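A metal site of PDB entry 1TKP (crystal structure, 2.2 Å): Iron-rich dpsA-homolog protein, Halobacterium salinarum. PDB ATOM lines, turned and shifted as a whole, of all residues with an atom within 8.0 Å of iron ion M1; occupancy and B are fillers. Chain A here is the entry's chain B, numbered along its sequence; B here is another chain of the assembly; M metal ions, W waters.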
ATOM      1  N   GLU A  75      31.352  -8.325 -13.075  1.00  0.00           N
ATOM      2  CA  GLU A  75      31.335  -7.017 -12.430  1.00  0.00           C
ATOM      3  C   GLU A  75      30.575  -5.961 -13.233  1.00  0.00           C
ATOM      4  O   GLU A  75      29.889  -5.098 -12.665  1.00  0.00           O
ATOM      5  CB  GLU A  75      32.721  -6.476 -12.160  1.00  0.00           C
ATOM      6  CG  GLU A  75      32.638  -5.233 -11.253  1.00  0.00           C
ATOM      7  CD  GLU A  75      33.975  -4.481 -11.114  1.00  0.00           C
ATOM      8  OE1 GLU A  75      34.993  -4.851 -11.850  1.00  0.00           O
ATOM      9  OE2 GLU A  75      33.998  -3.515 -10.272  1.00  0.00           O
ATOM     10  N   GLU A  76      30.745  -6.050 -14.538  1.00  0.00           N
ATOM     11  CA  GLU A  76      30.162  -5.133 -15.461  1.00  0.00           C
ATOM     12  C   GLU A  76      28.674  -5.414 -15.536  1.00  0.00           C
ATOM     13  O   GLU A  76      27.888  -4.457 -15.629  1.00  0.00           O
ATOM     14  CB  GLU A  76      30.744  -5.265 -16.850  1.00  0.00           C
ATOM     15  CG  GLU A  76      32.231  -5.112 -16.752  1.00  0.00           C
ATOM     16  CD  GLU A  76      32.920  -4.856 -18.074  1.00  0.00           C
ATOM     17  OE1 GLU A  76      32.153  -4.685 -19.107  1.00  0.00           O
ATOM     18  OE2 GLU A  76      34.210  -4.762 -18.052  1.00  0.00           O
ATOM     19  N   ALA A  78      26.924  -6.770 -13.149  1.00  0.00           N
ATOM     20  CA  ALA A  78      26.404  -6.222 -11.920  1.00  0.00           C
ATOM     21  C   ALA A  78      26.192  -4.733 -12.047  1.00  0.00           C
ATOM     22  O   ALA A  78      25.126  -4.164 -11.677  1.00  0.00           O
ATOM     23  CB  ALA A  78      27.425  -6.495 -10.755  1.00  0.00           C
ATOM     24  N   ASP A  79      27.225  -4.049 -12.567  1.00  0.00           N
ATOM     25  CA  ASP A  79      27.093  -2.626 -12.683  1.00  0.00           C
ATOM     26  C   ASP A  79      25.876  -2.280 -13.586  1.00  0.00           C
ATOM     27  O   ASP A  79      25.178  -1.405 -13.311  1.00  0.00           O
ATOM     28  CB  ASP A  79      28.377  -2.020 -13.295  1.00  0.00           C
ATOM     29  CG  ASP A  79      28.336  -0.515 -13.335  1.00  0.00           C
ATOM     30  OD1 ASP A  79      28.470   0.076 -12.244  1.00  0.00           O
ATOM     31  OD2 ASP A  79      28.159   0.178 -14.378  1.00  0.00           O
ATOM     32  N   GLU A  80      25.696  -2.924 -14.717  1.00  0.00           N
ATOM     33  CA  GLU A  80      24.591  -2.580 -15.552  1.00  0.00           C
ATOM     34  C   GLU A  80      23.226  -2.829 -14.832  1.00  0.00           C
ATOM     35  O   GLU A  80      22.342  -2.008 -14.945  1.00  0.00           O
ATOM     36  CB  GLU A  80      24.669  -3.338 -16.911  1.00  0.00           C
ATOM     37  CG  GLU A  80      25.618  -2.759 -18.069  1.00  0.00           C
ATOM     38  CD  GLU A  80      25.256  -1.391 -18.792  1.00  0.00           C
ATOM     39  OE1 GLU A  80      26.227  -0.532 -18.998  1.00  0.00           O
ATOM     40  OE2 GLU A  80      24.066  -1.134 -19.297  1.00  0.00           O
ATOM     41  N   ALA A  82      22.663  -2.868 -11.438  1.00  0.00           N
ATOM     42  CA  ALA A  82      22.405  -1.971 -10.353  1.00  0.00           C
ATOM     43  C   ALA A  82      21.996  -0.657 -10.960  1.00  0.00           C
ATOM     44  O   ALA A  82      21.087   0.019 -10.487  1.00  0.00           O
ATOM     45  CB  ALA A  82      23.618  -1.724  -9.526  1.00  0.00           C
ATOM     46  N   GLU A  83      22.634  -0.261 -12.032  1.00  0.00           N
ATOM     47  CA  GLU A  83      22.261   1.024 -12.598  1.00  0.00           C
ATOM     48  C   GLU A  83      20.870   1.044 -13.173  1.00  0.00           C
ATOM     49  O   GLU A  83      20.224   2.048 -13.149  1.00  0.00           O
ATOM     50  CB  GLU A  83      23.273   1.463 -13.633  1.00  0.00           C
ATOM     51  CG  GLU A  83      24.486   1.978 -12.846  1.00  0.00           C
ATOM     52  CD  GLU A  83      25.647   2.225 -13.751  1.00  0.00           C
ATOM     53  OE1 GLU A  83      26.696   2.699 -13.261  1.00  0.00           O
ATOM     54  OE2 GLU A  83      25.476   1.900 -14.957  1.00  0.00           O
ATOM     55  N   LYS B  49      30.876   2.074  -5.252  1.00  0.00           N
ATOM     56  CA  LYS B  49      29.895   1.645  -6.269  1.00  0.00           C
ATOM     57  C   LYS B  49      28.497   2.153  -5.908  1.00  0.00           C
ATOM     58  O   LYS B  49      27.752   2.735  -6.707  1.00  0.00           O
ATOM     59  CB  LYS B  49      29.858   0.125  -6.363  1.00  0.00           C
ATOM     60  CG  LYS B  49      31.024  -0.547  -7.001  1.00  0.00           C
ATOM     61  CD  LYS B  49      31.392  -0.025  -8.336  1.00  0.00           C
ATOM     62  CE  LYS B  49      30.513  -0.391  -9.397  1.00  0.00           C
ATOM     63  NZ  LYS B  49      31.330  -0.492 -10.784  1.00  0.00           N
ATOM     64  N   HIS B  52      28.282   5.781  -6.616  1.00  0.00           N
ATOM     65  CA  HIS B  52      28.315   5.939  -8.034  1.00  0.00           C
ATOM     66  C   HIS B  52      26.976   5.654  -8.691  1.00  0.00           C
ATOM     67  O   HIS B  52      26.505   6.502  -9.467  1.00  0.00           O
ATOM     68  CB  HIS B  52      29.429   4.940  -8.484  1.00  0.00           C
ATOM     69  CG  HIS B  52      29.447   4.590  -9.934  1.00  0.00           C
ATOM     70  ND1 HIS B  52      30.065   5.379 -10.894  1.00  0.00           N
ATOM     71  CD2 HIS B  52      29.126   3.430 -10.550  1.00  0.00           C
ATOM     72  CE1 HIS B  52      30.041   4.745 -12.062  1.00  0.00           C
ATOM     73  NE2 HIS B  52      29.509   3.538 -11.867  1.00  0.00           N
ATOM     74  N   TRP B  53      26.410   4.460  -8.440  1.00  0.00           N
ATOM     75  CA  TRP B  53      25.015   4.173  -8.788  1.00  0.00           C
ATOM     76  C   TRP B  53      24.051   5.246  -8.413  1.00  0.00           C
ATOM     77  O   TRP B  53      23.269   5.646  -9.248  1.00  0.00           O
ATOM     78  CB  TRP B  53      24.464   2.924  -8.127  1.00  0.00           C
ATOM     79  CG  TRP B  53      25.343   1.730  -8.567  1.00  0.00           C
ATOM     80  CD1 TRP B  53      26.113   1.621  -9.716  1.00  0.00           C
ATOM     81  CD2 TRP B  53      25.522   0.550  -7.861  1.00  0.00           C
ATOM     82  NE1 TRP B  53      26.755   0.409  -9.757  1.00  0.00           N
ATOM     83  CE2 TRP B  53      26.388  -0.283  -8.626  1.00  0.00           C
ATOM     84  CE3 TRP B  53      24.994   0.056  -6.665  1.00  0.00           C
ATOM     85  CZ2 TRP B  53      26.764  -1.540  -8.201  1.00  0.00           C
ATOM     86  CZ3 TRP B  53      25.358  -1.174  -6.248  1.00  0.00           C
ATOM     87  CH2 TRP B  53      26.250  -1.960  -7.004  1.00  0.00           C
ATOM     88  N   HIS B  64      29.747  10.725 -10.573  1.00  0.00           N
ATOM     89  CA  HIS B  64      29.390   9.388 -11.009  1.00  0.00           C
ATOM     90  C   HIS B  64      30.657   8.866 -11.663  1.00  0.00           C
ATOM     91  O   HIS B  64      31.106   7.742 -11.467  1.00  0.00           O
ATOM     92  CB  HIS B  64      28.214   9.451 -12.021  1.00  0.00           C
ATOM     93  CG  HIS B  64      27.907   8.147 -12.650  1.00  0.00           C
ATOM     94  ND1 HIS B  64      27.128   7.193 -12.037  1.00  0.00           N
ATOM     95  CD2 HIS B  64      28.257   7.625 -13.852  1.00  0.00           C
ATOM     96  CE1 HIS B  64      27.102   6.088 -12.769  1.00  0.00           C
ATOM     97  NE2 HIS B  64      27.765   6.334 -13.893  1.00  0.00           N
ATOM     98  N   LEU B  65      31.333   9.742 -12.363  1.00  0.00           N
ATOM     99  CA  LEU B  65      32.503   9.226 -12.971  1.00  0.00           C
ATOM    100  C   LEU B  65      33.612   9.173 -11.944  1.00  0.00           C
ATOM    101  O   LEU B  65      34.375   8.253 -11.965  1.00  0.00           O
ATOM    102  CB  LEU B  65      32.910  10.120 -14.082  1.00  0.00           C
ATOM    103  CG  LEU B  65      31.920  10.153 -15.233  1.00  0.00           C
ATOM    104  CD1 LEU B  65      32.298  11.294 -16.256  1.00  0.00           C
ATOM    105  CD2 LEU B  65      31.779   8.733 -15.845  1.00  0.00           C
ATOM    106  N   LEU B  67      33.386   8.519  -8.806  1.00  0.00           N
ATOM    107  CA  LEU B  67      33.190   7.512  -7.811  1.00  0.00           C
ATOM    108  C   LEU B  67      33.378   6.173  -8.502  1.00  0.00           C
ATOM    109  O   LEU B  67      33.875   5.207  -7.901  1.00  0.00           O
ATOM    110  CB  LEU B  67      31.796   7.725  -7.195  1.00  0.00           C
ATOM    111  CG  LEU B  67      31.586   8.907  -6.276  1.00  0.00           C
ATOM    112  CD1 LEU B  67      30.109   8.928  -5.975  1.00  0.00           C
ATOM    113  CD2 LEU B  67      32.252   8.578  -4.947  1.00  0.00           C
ATOM    114  N   GLY B  68      33.137   6.089  -9.817  1.00  0.00           N
ATOM    115  CA  GLY B  68      33.366   4.808 -10.521  1.00  0.00           C
ATOM    116  C   GLY B  68      34.860   4.550 -10.696  1.00  0.00           C
ATOM    117  O   GLY B  68      35.352   3.448 -10.525  1.00  0.00           O
HETATM  118 FE    FE M   1      28.706   2.117 -13.441  1.00  0.00          FE
HETATM  119 FE    FE M   2      21.920   4.785 -12.736  1.00  0.00          FE
HETATM  120  O   HOH W   1      28.998   3.572 -15.048  1.00  0.00           O
HETATM  121  O   HOH W   2      30.742   1.420 -13.589  1.00  0.00           O
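Iron ion M1 is bound by OE1 of Glu 83, water W2, water W1, OD2 of Asp 79, NE2 of His 52 of chain B and OD1 of Asp 79.
Iron ion M1 has six donor atoms within binding distance.
The backbone NH of Gly 68 of chain B lies within hydrogen-bond range of a ring nitrogen (ND1) of His 52 of chain B, 3.3 Å away.
NE1 of Trp 53 of chain B lies close to OD1 of Asp 79, 3.0 Å away.
A ring nitrogen (ND1) of His 52 of chain B sits at hydrogen-bond distance from the backbone carbonyl oxygen (O) of His 64 of chain B, at 2.6 Å.
The side-chain amino group (NZ) of Lys 49 of chain B sits close to the side-chain carboxylate (OD1) of Asp 79, at 3.3 Å.
The nearest printed residue that does not touch iron ion M1 is His 64 of chain B (4.3 Å).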
